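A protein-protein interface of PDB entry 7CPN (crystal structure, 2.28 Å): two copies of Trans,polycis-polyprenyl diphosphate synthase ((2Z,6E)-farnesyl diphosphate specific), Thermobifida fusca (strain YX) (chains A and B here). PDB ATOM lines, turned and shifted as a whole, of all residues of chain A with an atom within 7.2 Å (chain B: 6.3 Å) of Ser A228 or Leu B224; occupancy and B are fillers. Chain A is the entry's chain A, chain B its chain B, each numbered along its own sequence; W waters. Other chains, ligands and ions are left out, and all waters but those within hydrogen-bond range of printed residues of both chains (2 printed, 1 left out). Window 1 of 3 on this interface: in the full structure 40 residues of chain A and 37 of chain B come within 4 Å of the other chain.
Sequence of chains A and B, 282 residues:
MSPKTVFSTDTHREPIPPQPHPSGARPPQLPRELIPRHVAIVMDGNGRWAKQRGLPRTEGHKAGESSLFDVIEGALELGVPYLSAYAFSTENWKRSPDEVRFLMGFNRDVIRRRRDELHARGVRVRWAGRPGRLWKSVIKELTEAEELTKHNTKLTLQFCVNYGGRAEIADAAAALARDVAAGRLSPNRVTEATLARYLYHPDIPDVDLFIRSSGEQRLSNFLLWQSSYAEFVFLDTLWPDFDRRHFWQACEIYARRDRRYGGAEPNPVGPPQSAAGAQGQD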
ATOM      1  N   ARG A 166     -27.208 -12.606  13.375  1.00  0.00           N
ATOM      2  CA  ARG A 166     -27.167 -13.629  14.452  1.00  0.00           C
ATOM      3  C   ARG A 166     -28.581 -14.040  14.878  1.00  0.00           C
ATOM      4  O   ARG A 166     -28.820 -15.253  15.038  1.00  0.00           O
ATOM      5  CB  ARG A 166     -26.373 -13.094  15.631  1.00  0.00           C
ATOM      6  CG  ARG A 166     -24.884 -13.084  15.380  1.00  0.00           C
ATOM      7  CD  ARG A 166     -24.220 -12.802  16.690  1.00  0.00           C
ATOM      8  NE  ARG A 166     -22.790 -12.825  16.591  1.00  0.00           N
ATOM      9  CZ  ARG A 166     -21.987 -12.616  17.625  1.00  0.00           C
ATOM     10  NH1 ARG A 166     -22.502 -12.388  18.810  1.00  0.00           N
ATOM     11  NH2 ARG A 166     -20.678 -12.667  17.489  1.00  0.00           N
ATOM     12  N   ILE A 169     -30.061 -16.393  12.227  1.00  0.00           N
ATOM     13  CA  ILE A 169     -29.434 -17.741  12.323  1.00  0.00           C
ATOM     14  C   ILE A 169     -29.970 -18.493  13.555  1.00  0.00           C
ATOM     15  O   ILE A 169     -30.234 -19.709  13.451  1.00  0.00           O
ATOM     16  CB  ILE A 169     -27.908 -17.587  12.333  1.00  0.00           C
ATOM     17  CG1 ILE A 169     -27.427 -17.040  10.983  1.00  0.00           C
ATOM     18  CG2 ILE A 169     -27.236 -18.907  12.677  1.00  0.00           C
ATOM     19  CD1 ILE A 169     -26.026 -16.572  10.980  1.00  0.00           C
ATOM     20  N   ASP A 206     -27.920 -15.594  -1.931  1.00  0.00           N
ATOM     21  CA  ASP A 206     -26.716 -15.005  -1.311  1.00  0.00           C
ATOM     22  C   ASP A 206     -26.577 -13.551  -1.735  1.00  0.00           C
ATOM     23  O   ASP A 206     -27.000 -13.230  -2.851  1.00  0.00           O
ATOM     24  CB  ASP A 206     -25.448 -15.745  -1.731  1.00  0.00           C
ATOM     25  CG  ASP A 206     -25.361 -17.163  -1.204  1.00  0.00           C
ATOM     26  OD1 ASP A 206     -26.056 -17.463  -0.182  1.00  0.00           O
ATOM     27  OD2 ASP A 206     -24.619 -17.970  -1.839  1.00  0.00           O
ATOM     28  N   VAL A 207     -25.991 -12.726  -0.868  1.00  0.00           N
ATOM     29  CA  VAL A 207     -25.596 -11.328  -1.213  1.00  0.00           C
ATOM     30  C   VAL A 207     -24.357 -11.407  -2.098  1.00  0.00           C
ATOM     31  O   VAL A 207     -23.388 -12.089  -1.708  1.00  0.00           O
ATOM     32  CB  VAL A 207     -25.353 -10.494   0.042  1.00  0.00           C
ATOM     33  CG1 VAL A 207     -24.825  -9.116  -0.302  1.00  0.00           C
ATOM     34  CG2 VAL A 207     -26.608 -10.384   0.868  1.00  0.00           C
ATOM     35  N   LEU A 219     -19.736  -5.016   9.069  1.00  0.00           N
ATOM     36  CA  LEU A 219     -20.973  -5.676   8.577  1.00  0.00           C
ATOM     37  C   LEU A 219     -22.149  -5.186   9.428  1.00  0.00           C
ATOM     38  O   LEU A 219     -23.291  -5.200   8.937  1.00  0.00           O
ATOM     39  CB  LEU A 219     -20.793  -7.191   8.721  1.00  0.00           C
ATOM     40  CG  LEU A 219     -21.762  -8.074   7.940  1.00  0.00           C
ATOM     41  CD1 LEU A 219     -21.365  -8.219   6.488  1.00  0.00           C
ATOM     42  CD2 LEU A 219     -21.828  -9.444   8.564  1.00  0.00           C
ATOM     43  N   ASN A 221     -23.659  -6.809  11.639  1.00  0.00           N
ATOM     44  CA  ASN A 221     -24.606  -7.909  11.954  1.00  0.00           C
ATOM     45  C   ASN A 221     -25.716  -7.919  10.918  1.00  0.00           C
ATOM     46  O   ASN A 221     -26.893  -8.065  11.343  1.00  0.00           O
ATOM     47  CB  ASN A 221     -25.179  -7.737  13.369  1.00  0.00           C
ATOM     48  CG  ASN A 221     -25.898  -8.968  13.892  1.00  0.00           C
ATOM     49  OD1 ASN A 221     -25.570 -10.090  13.489  1.00  0.00           O
ATOM     50  ND2 ASN A 221     -26.888  -8.769  14.753  1.00  0.00           N
ATOM     51  N   LEU A 223     -27.271  -9.599   7.346  1.00  0.00           N
ATOM     52  CA  LEU A 223     -27.271 -10.753   6.399  1.00  0.00           C
ATOM     53  C   LEU A 223     -25.947 -11.536   6.466  1.00  0.00           C
ATOM     54  O   LEU A 223     -25.302 -11.826   5.426  1.00  0.00           O
ATOM     55  CB  LEU A 223     -27.513 -10.234   4.991  1.00  0.00           C
ATOM     56  CG  LEU A 223     -28.876  -9.579   4.798  1.00  0.00           C
ATOM     57  CD1 LEU A 223     -28.996  -9.017   3.401  1.00  0.00           C
ATOM     58  CD2 LEU A 223     -29.993 -10.578   5.075  1.00  0.00           C
ATOM     59  N   LEU A 224     -25.636 -11.968   7.671  1.00  0.00           N
ATOM     60  CA  LEU A 224     -24.370 -12.660   8.012  1.00  0.00           C
ATOM     61  C   LEU A 224     -24.221 -13.968   7.221  1.00  0.00           C
ATOM     62  O   LEU A 224     -23.227 -14.139   6.517  1.00  0.00           O
ATOM     63  CB  LEU A 224     -24.475 -12.895   9.509  1.00  0.00           C
ATOM     64  CG  LEU A 224     -23.185 -13.084  10.271  1.00  0.00           C
ATOM     65  CD1 LEU A 224     -22.152 -12.053   9.902  1.00  0.00           C
ATOM     66  CD2 LEU A 224     -23.502 -12.925  11.745  1.00  0.00           C
ATOM     67  N   TRP A 225     -25.186 -14.871   7.294  1.00  0.00           N
ATOM     68  CA  TRP A 225     -25.098 -16.152   6.560  1.00  0.00           C
ATOM     69  C   TRP A 225     -24.964 -15.840   5.069  1.00  0.00           C
ATOM     70  O   TRP A 225     -24.111 -16.448   4.407  1.00  0.00           O
ATOM     71  CB  TRP A 225     -26.337 -16.998   6.829  1.00  0.00           C
ATOM     72  CG  TRP A 225     -26.347 -18.294   6.090  1.00  0.00           C
ATOM     73  CD1 TRP A 225     -26.807 -18.526   4.828  1.00  0.00           C
ATOM     74  CD2 TRP A 225     -25.916 -19.557   6.610  1.00  0.00           C
ATOM     75  NE1 TRP A 225     -26.722 -19.865   4.543  1.00  0.00           N
ATOM     76  CE2 TRP A 225     -26.202 -20.527   5.625  1.00  0.00           C
ATOM     77  CE3 TRP A 225     -25.409 -19.971   7.839  1.00  0.00           C
ATOM     78  CZ2 TRP A 225     -25.932 -21.885   5.813  1.00  0.00           C
ATOM     79  CZ3 TRP A 225     -25.121 -21.309   8.012  1.00  0.00           C
ATOM     80  CH2 TRP A 225     -25.372 -22.244   7.011  1.00  0.00           C
ATOM     81  N   GLN A 226     -25.800 -14.929   4.581  1.00  0.00           N
ATOM     82  CA  GLN A 226     -26.004 -14.649   3.138  1.00  0.00           C
ATOM     83  C   GLN A 226     -24.785 -13.906   2.545  1.00  0.00           C
ATOM     84  O   GLN A 226     -24.616 -13.990   1.315  1.00  0.00           O
ATOM     85  CB  GLN A 226     -27.314 -13.883   2.963  1.00  0.00           C
ATOM     86  CG  GLN A 226     -28.548 -14.610   3.514  1.00  0.00           C
ATOM     87  CD  GLN A 226     -28.900 -14.271   4.954  1.00  0.00           C
ATOM     88  OE1 GLN A 226     -28.054 -13.911   5.773  1.00  0.00           O
ATOM     89  NE2 GLN A 226     -30.182 -14.365   5.259  1.00  0.00           N
ATOM     90  N   SER A 227     -23.945 -13.262   3.370  1.00  0.00           N
ATOM     91  CA  SER A 227     -22.861 -12.349   2.921  1.00  0.00           C
ATOM     92  C   SER A 227     -21.499 -13.056   2.960  1.00  0.00           C
ATOM     93  O   SER A 227     -20.490 -12.394   2.717  1.00  0.00           O
ATOM     94  CB  SER A 227     -22.852 -11.086   3.733  1.00  0.00           C
ATOM     95  OG  SER A 227     -24.027 -10.334   3.470  1.00  0.00           O
ATOM     96  N   SER A 228     -21.481 -14.347   3.240  1.00  0.00           N
ATOM     97  CA  SER A 228     -20.263 -15.171   3.407  1.00  0.00           C
ATOM     98  C   SER A 228     -19.239 -14.922   2.298  1.00  0.00           C
ATOM     99  O   SER A 228     -18.030 -14.894   2.619  1.00  0.00           O
ATOM    100  CB  SER A 228     -20.640 -16.653   3.389  1.00  0.00           C
ATOM    101  OG  SER A 228     -19.563 -17.463   3.855  1.00  0.00           O
ATOM    102  N   TYR A 229     -19.691 -14.842   1.045  1.00  0.00           N
ATOM    103  CA  TYR A 229     -18.804 -14.632  -0.130  1.00  0.00           C
ATOM    104  C   TYR A 229     -19.114 -13.313  -0.850  1.00  0.00           C
ATOM    105  O   TYR A 229     -18.630 -13.119  -1.955  1.00  0.00           O
ATOM    106  CB  TYR A 229     -18.847 -15.864  -1.035  1.00  0.00           C
ATOM    107  CG  TYR A 229     -17.819 -16.869  -0.577  1.00  0.00           C
ATOM    108  CD1 TYR A 229     -16.466 -16.580  -0.711  1.00  0.00           C
ATOM    109  CD2 TYR A 229     -18.172 -18.059   0.029  1.00  0.00           C
ATOM    110  CE1 TYR A 229     -15.487 -17.467  -0.288  1.00  0.00           C
ATOM    111  CE2 TYR A 229     -17.206 -18.948   0.481  1.00  0.00           C
ATOM    112  CZ  TYR A 229     -15.860 -18.653   0.329  1.00  0.00           C
ATOM    113  OH  TYR A 229     -14.906 -19.537   0.775  1.00  0.00           O
ATOM    114  N   ALA A 230     -19.802 -12.391  -0.202  1.00  0.00           N
ATOM    115  CA  ALA A 230     -20.155 -11.074  -0.772  1.00  0.00           C
ATOM    116  C   ALA A 230     -18.916 -10.193  -0.957  1.00  0.00           C
ATOM    117  O   ALA A 230     -18.026 -10.213  -0.108  1.00  0.00           O
ATOM    118  CB  ALA A 230     -21.144 -10.364   0.108  1.00  0.00           C
ATOM    119  N   GLU A 231     -18.916  -9.386  -2.017  1.00  0.00           N
ATOM    120  CA  GLU A 231     -17.946  -8.285  -2.221  1.00  0.00           C
ATOM    121  C   GLU A 231     -18.400  -7.108  -1.385  1.00  0.00           C
ATOM    122  O   GLU A 231     -19.580  -6.752  -1.473  1.00  0.00           O
ATOM    123  CB  GLU A 231     -17.852  -7.878  -3.694  1.00  0.00           C
ATOM    124  CG  GLU A 231     -17.242  -8.927  -4.592  1.00  0.00           C
ATOM    125  CD  GLU A 231     -15.779  -9.255  -4.278  1.00  0.00           C
ATOM    126  OE1 GLU A 231     -15.067  -8.338  -3.800  1.00  0.00           O
ATOM    127  OE2 GLU A 231     -15.370 -10.452  -4.444  1.00  0.00           O
ATOM    128  N   PHE A 232     -17.503  -6.547  -0.573  1.00  0.00           N
ATOM    129  CA  PHE A 232     -17.802  -5.339   0.234  1.00  0.00           C
ATOM    130  C   PHE A 232     -17.289  -4.113  -0.532  1.00  0.00           C
ATOM    131  O   PHE A 232     -16.165  -4.146  -1.038  1.00  0.00           O
ATOM    132  CB  PHE A 232     -17.173  -5.456   1.619  1.00  0.00           C
ATOM    133  CG  PHE A 232     -17.911  -6.446   2.476  1.00  0.00           C
ATOM    134  CD1 PHE A 232     -17.809  -7.810   2.248  1.00  0.00           C
ATOM    135  CD2 PHE A 232     -18.738  -5.999   3.486  1.00  0.00           C
ATOM    136  CE1 PHE A 232     -18.528  -8.709   3.015  1.00  0.00           C
ATOM    137  CE2 PHE A 232     -19.434  -6.904   4.271  1.00  0.00           C
ATOM    138  CZ  PHE A 232     -19.321  -8.256   4.040  1.00  0.00           C
ATOM    139  N   ARG A 259     -14.104 -12.509  -8.229  1.00  0.00           N
ATOM    140  CA  ARG A 259     -14.808 -13.467  -7.321  1.00  0.00           C
ATOM    141  C   ARG A 259     -14.299 -14.906  -7.535  1.00  0.00           C
ATOM    142  O   ARG A 259     -14.399 -15.399  -8.665  1.00  0.00           O
ATOM    143  CB  ARG A 259     -16.316 -13.392  -7.556  1.00  0.00           C
ATOM    144  CG  ARG A 259     -16.871 -11.980  -7.510  1.00  0.00           C
ATOM    145  CD  ARG A 259     -18.386 -11.991  -7.369  1.00  0.00           C
ATOM    146  NE  ARG A 259     -18.779 -12.353  -6.008  1.00  0.00           N
ATOM    147  CZ  ARG A 259     -20.017 -12.649  -5.610  1.00  0.00           C
ATOM    148  NH1 ARG A 259     -21.031 -12.657  -6.466  1.00  0.00           N
ATOM    149  NH2 ARG A 259     -20.218 -12.997  -4.354  1.00  0.00           N
ATOM    150  N   GLU B  91     -13.585 -24.331   0.942  1.00  0.00           N
ATOM    151  CA  GLU B  91     -13.696 -23.946  -0.482  1.00  0.00           C
ATOM    152  C   GLU B  91     -12.371 -24.207  -1.223  1.00  0.00           C
ATOM    153  O   GLU B  91     -12.356 -24.166  -2.455  1.00  0.00           O
ATOM    154  CB  GLU B  91     -14.208 -22.499  -0.547  1.00  0.00           C
ATOM    155  CG  GLU B  91     -15.718 -22.354  -0.229  1.00  0.00           C
ATOM    156  CD  GLU B  91     -16.194 -22.396   1.232  1.00  0.00           C
ATOM    157  OE1 GLU B  91     -17.188 -23.131   1.495  1.00  0.00           O
ATOM    158  OE2 GLU B  91     -15.572 -21.711   2.135  1.00  0.00           O
ATOM    159  N   TYR B 163     -11.871 -25.461   7.397  1.00  0.00           N
ATOM    160  CA  TYR B 163     -12.794 -24.563   8.126  1.00  0.00           C
ATOM    161  C   TYR B 163     -13.688 -23.789   7.153  1.00  0.00           C
ATOM    162  O   TYR B 163     -13.168 -23.297   6.128  1.00  0.00           O
ATOM    163  CB  TYR B 163     -12.031 -23.606   9.033  1.00  0.00           C
ATOM    164  CG  TYR B 163     -12.957 -22.642   9.720  1.00  0.00           C
ATOM    165  CD1 TYR B 163     -13.357 -21.473   9.088  1.00  0.00           C
ATOM    166  CD2 TYR B 163     -13.536 -22.945  10.942  1.00  0.00           C
ATOM    167  CE1 TYR B 163     -14.274 -20.618   9.671  1.00  0.00           C
ATOM    168  CE2 TYR B 163     -14.426 -22.086  11.556  1.00  0.00           C
ATOM    169  CZ  TYR B 163     -14.815 -20.925  10.904  1.00  0.00           C
ATOM    170  OH  TYR B 163     -15.760 -20.111  11.445  1.00  0.00           O
ATOM    171  N   GLY B 165     -17.195 -20.846   7.865  1.00  0.00           N
ATOM    172  CA  GLY B 165     -18.087 -20.169   8.830  1.00  0.00           C
ATOM    173  C   GLY B 165     -19.458 -20.794   8.834  1.00  0.00           C
ATOM    174  O   GLY B 165     -19.989 -21.068   9.930  1.00  0.00           O
ATOM    175  N   ARG B 166     -20.026 -20.986   7.654  1.00  0.00           N
ATOM    176  CA  ARG B 166     -21.326 -21.695   7.483  1.00  0.00           C
ATOM    177  C   ARG B 166     -21.232 -23.138   8.008  1.00  0.00           C
ATOM    178  O   ARG B 166     -22.165 -23.564   8.690  1.00  0.00           O
ATOM    179  CB  ARG B 166     -21.721 -21.688   6.017  1.00  0.00           C
ATOM    180  CG  ARG B 166     -22.177 -20.323   5.535  1.00  0.00           C
ATOM    181  CD  ARG B 166     -22.778 -20.526   4.170  1.00  0.00           C
ATOM    182  NE  ARG B 166     -23.294 -19.281   3.632  1.00  0.00           N
ATOM    183  CZ  ARG B 166     -23.818 -19.169   2.436  1.00  0.00           C
ATOM    184  NH1 ARG B 166     -23.905 -20.237   1.670  1.00  0.00           N
ATOM    185  NH2 ARG B 166     -24.273 -18.005   2.004  1.00  0.00           N
ATOM    186  N   GLU B 168     -19.289 -24.264  10.357  1.00  0.00           N
ATOM    187  CA  GLU B 168     -19.224 -24.162  11.837  1.00  0.00           C
ATOM    188  C   GLU B 168     -20.618 -23.944  12.415  1.00  0.00           C
ATOM    189  O   GLU B 168     -20.952 -24.587  13.414  1.00  0.00           O
ATOM    190  CB  GLU B 168     -18.264 -23.071  12.297  1.00  0.00           C
ATOM    191  CG  GLU B 168     -18.060 -23.058  13.794  1.00  0.00           C
ATOM    192  CD  GLU B 168     -17.154 -21.956  14.341  1.00  0.00           C
ATOM    193  OE1 GLU B 168     -16.877 -20.962  13.608  1.00  0.00           O
ATOM    194  OE2 GLU B 168     -16.739 -22.080  15.539  1.00  0.00           O
ATOM    195  N   ILE B 169     -21.383 -23.031  11.831  1.00  0.00           N
ATOM    196  CA  ILE B 169     -22.767 -22.726  12.271  1.00  0.00           C
ATOM    197  C   ILE B 169     -23.666 -23.944  12.079  1.00  0.00           C
ATOM    198  O   ILE B 169     -24.504 -24.216  12.973  1.00  0.00           O
ATOM    199  CB  ILE B 169     -23.266 -21.480  11.535  1.00  0.00           C
ATOM    200  CG1 ILE B 169     -22.463 -20.257  11.987  1.00  0.00           C
ATOM    201  CG2 ILE B 169     -24.757 -21.262  11.751  1.00  0.00           C
ATOM    202  CD1 ILE B 169     -22.641 -19.052  11.067  1.00  0.00           C
ATOM    203  N   ARG B 218     -13.575  -8.924   1.302  1.00  0.00           N
ATOM    204  CA  ARG B 218     -14.603  -9.983   1.535  1.00  0.00           C
ATOM    205  C   ARG B 218     -14.219 -10.841   2.742  1.00  0.00           C
ATOM    206  O   ARG B 218     -13.028 -10.850   3.142  1.00  0.00           O
ATOM    207  CB  ARG B 218     -14.841 -10.866   0.298  1.00  0.00           C
ATOM    208  CG  ARG B 218     -13.636 -11.054  -0.589  1.00  0.00           C
ATOM    209  CD  ARG B 218     -13.930 -11.911  -1.811  1.00  0.00           C
ATOM    210  NE  ARG B 218     -12.728 -12.554  -2.363  1.00  0.00           N
ATOM    211  CZ  ARG B 218     -12.134 -12.296  -3.555  1.00  0.00           C
ATOM    212  NH1 ARG B 218     -11.064 -12.989  -3.910  1.00  0.00           N
ATOM    213  NH2 ARG B 218     -12.607 -11.371  -4.379  1.00  0.00           N
ATOM    214  N   LEU B 219     -15.219 -11.501   3.327  1.00  0.00           N
ATOM    215  CA  LEU B 219     -15.047 -12.354   4.531  1.00  0.00           C
ATOM    216  C   LEU B 219     -14.538 -13.719   4.082  1.00  0.00           C
ATOM    217  O   LEU B 219     -13.820 -14.361   4.849  1.00  0.00           O
ATOM    218  CB  LEU B 219     -16.380 -12.502   5.261  1.00  0.00           C
ATOM    219  CG  LEU B 219     -16.695 -11.411   6.287  1.00  0.00           C
ATOM    220  CD1 LEU B 219     -18.105 -10.910   6.095  1.00  0.00           C
ATOM    221  CD2 LEU B 219     -16.535 -11.926   7.710  1.00  0.00           C
ATOM    222  N   SER B 220     -14.911 -14.139   2.884  1.00  0.00           N
ATOM    223  CA  SER B 220     -14.622 -15.500   2.360  1.00  0.00           C
ATOM    224  C   SER B 220     -14.987 -16.569   3.403  1.00  0.00           C
ATOM    225  O   SER B 220     -14.187 -17.487   3.617  1.00  0.00           O
ATOM    226  CB  SER B 220     -13.155 -15.598   1.963  1.00  0.00           C
ATOM    227  OG  SER B 220     -12.864 -14.648   0.935  1.00  0.00           O
ATOM    228  N   ASN B 221     -16.131 -16.425   4.063  1.00  0.00           N
ATOM    229  CA  ASN B 221     -16.718 -17.511   4.904  1.00  0.00           C
ATOM    230  C   ASN B 221     -15.805 -17.786   6.100  1.00  0.00           C
ATOM    231  O   ASN B 221     -15.618 -18.964   6.420  1.00  0.00           O
ATOM    232  CB  ASN B 221     -16.847 -18.802   4.081  1.00  0.00           C
ATOM    233  CG  ASN B 221     -17.781 -19.814   4.679  1.00  0.00           C
ATOM    234  OD1 ASN B 221     -18.688 -19.475   5.451  1.00  0.00           O
ATOM    235  ND2 ASN B 221     -17.546 -21.077   4.342  1.00  0.00           N
ATOM    236  N   PHE B 222     -15.144 -16.759   6.661  1.00  0.00           N
ATOM    237  CA  PHE B 222     -14.179 -16.892   7.784  1.00  0.00           C
ATOM    238  C   PHE B 222     -14.771 -16.283   9.066  1.00  0.00           C
ATOM    239  O   PHE B 222     -15.104 -15.078   9.094  1.00  0.00           O
ATOM    240  CB  PHE B 222     -12.838 -16.276   7.423  1.00  0.00           C
ATOM    241  CG  PHE B 222     -11.748 -16.479   8.453  1.00  0.00           C
ATOM    242  CD1 PHE B 222     -11.490 -17.731   8.994  1.00  0.00           C
ATOM    243  CD2 PHE B 222     -10.958 -15.414   8.856  1.00  0.00           C
ATOM    244  CE1 PHE B 222     -10.466 -17.917   9.913  1.00  0.00           C
ATOM    245  CE2 PHE B 222      -9.905 -15.612   9.746  1.00  0.00           C
ATOM    246  CZ  PHE B 222      -9.686 -16.861  10.302  1.00  0.00           C
ATOM    247  N   LEU B 223     -14.942 -17.133  10.085  1.00  0.00           N
ATOM    248  CA  LEU B 223     -15.448 -16.719  11.428  1.00  0.00           C
ATOM    249  C   LEU B 223     -16.644 -15.786  11.276  1.00  0.00           C
ATOM    250  O   LEU B 223     -16.709 -14.725  11.898  1.00  0.00           O
ATOM    251  CB  LEU B 223     -14.311 -16.068  12.214  1.00  0.00           C
ATOM    252  CG  LEU B 223     -13.149 -16.988  12.512  1.00  0.00           C
ATOM    253  CD1 LEU B 223     -12.049 -16.225  13.201  1.00  0.00           C
ATOM    254  CD2 LEU B 223     -13.627 -18.173  13.349  1.00  0.00           C
ATOM    255  N   LEU B 224     -17.625 -16.270  10.559  1.00  0.00           N
ATOM    256  CA  LEU B 224     -18.856 -15.547  10.183  1.00  0.00           C
ATOM    257  C   LEU B 224     -19.639 -15.110  11.418  1.00  0.00           C
ATOM    258  O   LEU B 224     -19.887 -13.913  11.605  1.00  0.00           O
ATOM    259  CB  LEU B 224     -19.662 -16.533   9.340  1.00  0.00           C
ATOM    260  CG  LEU B 224     -20.550 -15.914   8.293  1.00  0.00           C
ATOM    261  CD1 LEU B 224     -19.784 -14.874   7.466  1.00  0.00           C
ATOM    262  CD2 LEU B 224     -21.054 -17.035   7.378  1.00  0.00           C
ATOM    263  N   TRP B 225     -20.017 -16.052  12.287  1.00  0.00           N
ATOM    264  CA  TRP B 225     -20.766 -15.683  13.508  1.00  0.00           C
ATOM    265  C   TRP B 225     -19.937 -14.687  14.321  1.00  0.00           C
ATOM    266  O   TRP B 225     -20.505 -13.670  14.782  1.00  0.00           O
ATOM    267  CB  TRP B 225     -21.074 -16.927  14.314  1.00  0.00           C
ATOM    268  CG  TRP B 225     -21.801 -16.664  15.587  1.00  0.00           C
ATOM    269  CD1 TRP B 225     -21.268 -16.336  16.800  1.00  0.00           C
ATOM    270  CD2 TRP B 225     -23.220 -16.740  15.773  1.00  0.00           C
ATOM    271  NE1 TRP B 225     -22.264 -16.218  17.723  1.00  0.00           N
ATOM    272  CE2 TRP B 225     -23.473 -16.424  17.124  1.00  0.00           C
ATOM    273  CE3 TRP B 225     -24.301 -16.980  14.928  1.00  0.00           C
ATOM    274  CZ2 TRP B 225     -24.756 -16.394  17.654  1.00  0.00           C
ATOM    275  CZ3 TRP B 225     -25.564 -16.951  15.454  1.00  0.00           C
ATOM    276  CH2 TRP B 225     -25.778 -16.682  16.787  1.00  0.00           C
ATOM    277  N   GLN B 226     -18.654 -14.983  14.479  1.00  0.00           N
ATOM    278  CA  GLN B 226     -17.728 -14.297  15.415  1.00  0.00           C
ATOM    279  C   GLN B 226     -17.361 -12.893  14.897  1.00  0.00           C
ATOM    280  O   GLN B 226     -16.949 -12.066  15.743  1.00  0.00           O
ATOM    281  CB  GLN B 226     -16.488 -15.176  15.645  1.00  0.00           C
ATOM    282  CG  GLN B 226     -16.818 -16.568  16.206  1.00  0.00           C
ATOM    283  CD  GLN B 226     -17.009 -17.643  15.152  1.00  0.00           C
ATOM    284  OE1 GLN B 226     -17.408 -17.380  14.006  1.00  0.00           O
ATOM    285  NE2 GLN B 226     -16.654 -18.873  15.529  1.00  0.00           N
ATOM    286  N   SER B 227     -17.536 -12.607  13.599  1.00  0.00           N
ATOM    287  CA  SER B 227     -17.033 -11.365  12.949  1.00  0.00           C
ATOM    288  C   SER B 227     -18.176 -10.353  12.754  1.00  0.00           C
ATOM    289  O   SER B 227     -17.950  -9.331  12.132  1.00  0.00           O
ATOM    290  CB  SER B 227     -16.365 -11.680  11.652  1.00  0.00           C
ATOM    291  OG  SER B 227     -15.164 -12.395  11.904  1.00  0.00           O
ATOM    292  N   SER B 228     -19.348 -10.648  13.280  1.00  0.00           N
ATOM    293  CA  SER B 228     -20.590  -9.870  13.032  1.00  0.00           C
ATOM    294  C   SER B 228     -20.373  -8.364  13.283  1.00  0.00           C
ATOM    295  O   SER B 228     -20.986  -7.541  12.629  1.00  0.00           O
ATOM    296  CB  SER B 228     -21.688 -10.368  13.923  1.00  0.00           C
ATOM    297  OG  SER B 228     -22.910 -10.063  13.302  1.00  0.00           O
HETATM  298  O   HOH W   1     -12.488  -8.277  -3.238  1.00  0.00           O
HETATM  299  O   HOH W   2     -12.398 -19.526   1.412  1.00  0.00           O
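The side-chain amide oxygen (OD1) of Asn A221 lies within hydrogen-bond range of the side-chain hydroxyl (OG) of Ser B228. The side-chain carboxylate (OE2) of Glu A231 is in salt-bridge range of the guanidinium group (NH2) of Arg B218 (2.9 Å). OH of Tyr A229 lies within hydrogen-bond range of OE2 of Glu B91, 2.6 Å away. N of Ser B220 sits at hydrogen-bond distance from O of Ser A228 (3.2 Å). OG of Ser A228 sits at hydrogen-bond distance from OD1 of Asn B221 (2.7 Å). The backbone carbonyl oxygen (O) of Trp B225 lies within hydrogen-bond range of the guanidinium group (NH2) of Arg A166, 2.9 Å away. The backbone carbonyl oxygen (O) of Trp A225 lies within hydrogen-bond range of the guanidinium group (NH2) of Arg B166 (2.9 Å). The side-chain carboxylate (OD1) of Asp A206 lies within salt-bridge range of the guanidinium group (NH2) of Arg B166, 2.9 Å away.
Printed residues of chain A that touch a printed residue of chain B: Arg A166, Ile A169, Asp A206, Leu A219, Asn A221, Leu A224, Trp A225, Gln A226, Ser A228, Tyr A229, Ala A230, Glu A231 and Phe A232. Hydrophobic or aromatic side chains of chain A within 4 Å of the printed part of chain B: Ile A169, Leu A219, Leu A224, Trp A225, Tyr A229 and Phe A232. Among the printed residues, Asp or Glu carboxylates within 4 Å of a Lys or Arg side-chain nitrogen of the other chain: Asp A206 with Arg B166 (2.9 Å) and Glu A231 with Arg B218 (2.9 Å).
The backbone NH (N) of Val A207 sits at hydrogen-bond distance from the backbone carbonyl oxygen (O) of Gln A226, at 2.9 Å. The backbone NH (N) of Arg B166 is in hydrogen-bond range of the side-chain amide oxygen (OD1) of Asn B221 (3.0 Å).
Val A207 touches none of the printed residues of chain B. Printed residues of chain B within 4 Å of Gln A226: Arg B166. Of chain B, only Arg B166 (3.7 Å), Leu B219 (3.9 Å), Ser B220 (3.2 Å), Asn B221 (2.7 Å) and Leu B224 (3.8 Å) come within 4 Å of Ser A228. Of the printed residues of chain A, Leu B224 touches Leu A224 (3.4 Å) and Ser A228 (3.8 Å). The nearest residue of chain B that does not touch Ser A228 is Phe B222 (5.3 Å). The nearest residue of chain A that does not touch Leu B224 is Trp A225 (4.2 Å).
Leu A219 touches Ser B228, and with the chains exchanged Ser A228 touches Leu B219. Leu A224 touches its own counterpart, Leu B224.
Water W2 lies within hydrogen-bond range of OH of Tyr A229 and O of Ser B220. Water W1 lies within hydrogen-bond range of OE1 of Glu A231 (2.6 Å) and NH2 of Arg B218 (3.3 Å).
Among the printed residues, merely in contact across the chains: Ala A230 with Arg B218 (3.3 Å), Leu A224 with Ser B228 (3.3 Å), Leu A224 with Leu B224 (3.4 Å), Tyr A229 with Ser B220 (3.4 Å), Ile A169 with Ile B169 (3.5 Å), Phe A232 with Leu B219 (3.6 Å), Tyr A229 with Asn B221 (3.6 Å), Ser A228 with Arg B166 (3.7 Å), Trp A225 with Ile B169 (3.8 Å), Ile A169 with Trp B225 (3.8 Å), Arg A166 with Ser B228 (3.8 Å), Ser A228 with Leu B224 (3.8 Å), Ser A228 with Leu B219 (3.9 Å), Leu A219 with Ser B228 (3.9 Å), Phe A232 with Arg B218 (3.9 Å), Gln A226 with Arg B166 (3.9 Å) and Arg A166 with Gln B226 (3.96 Å).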
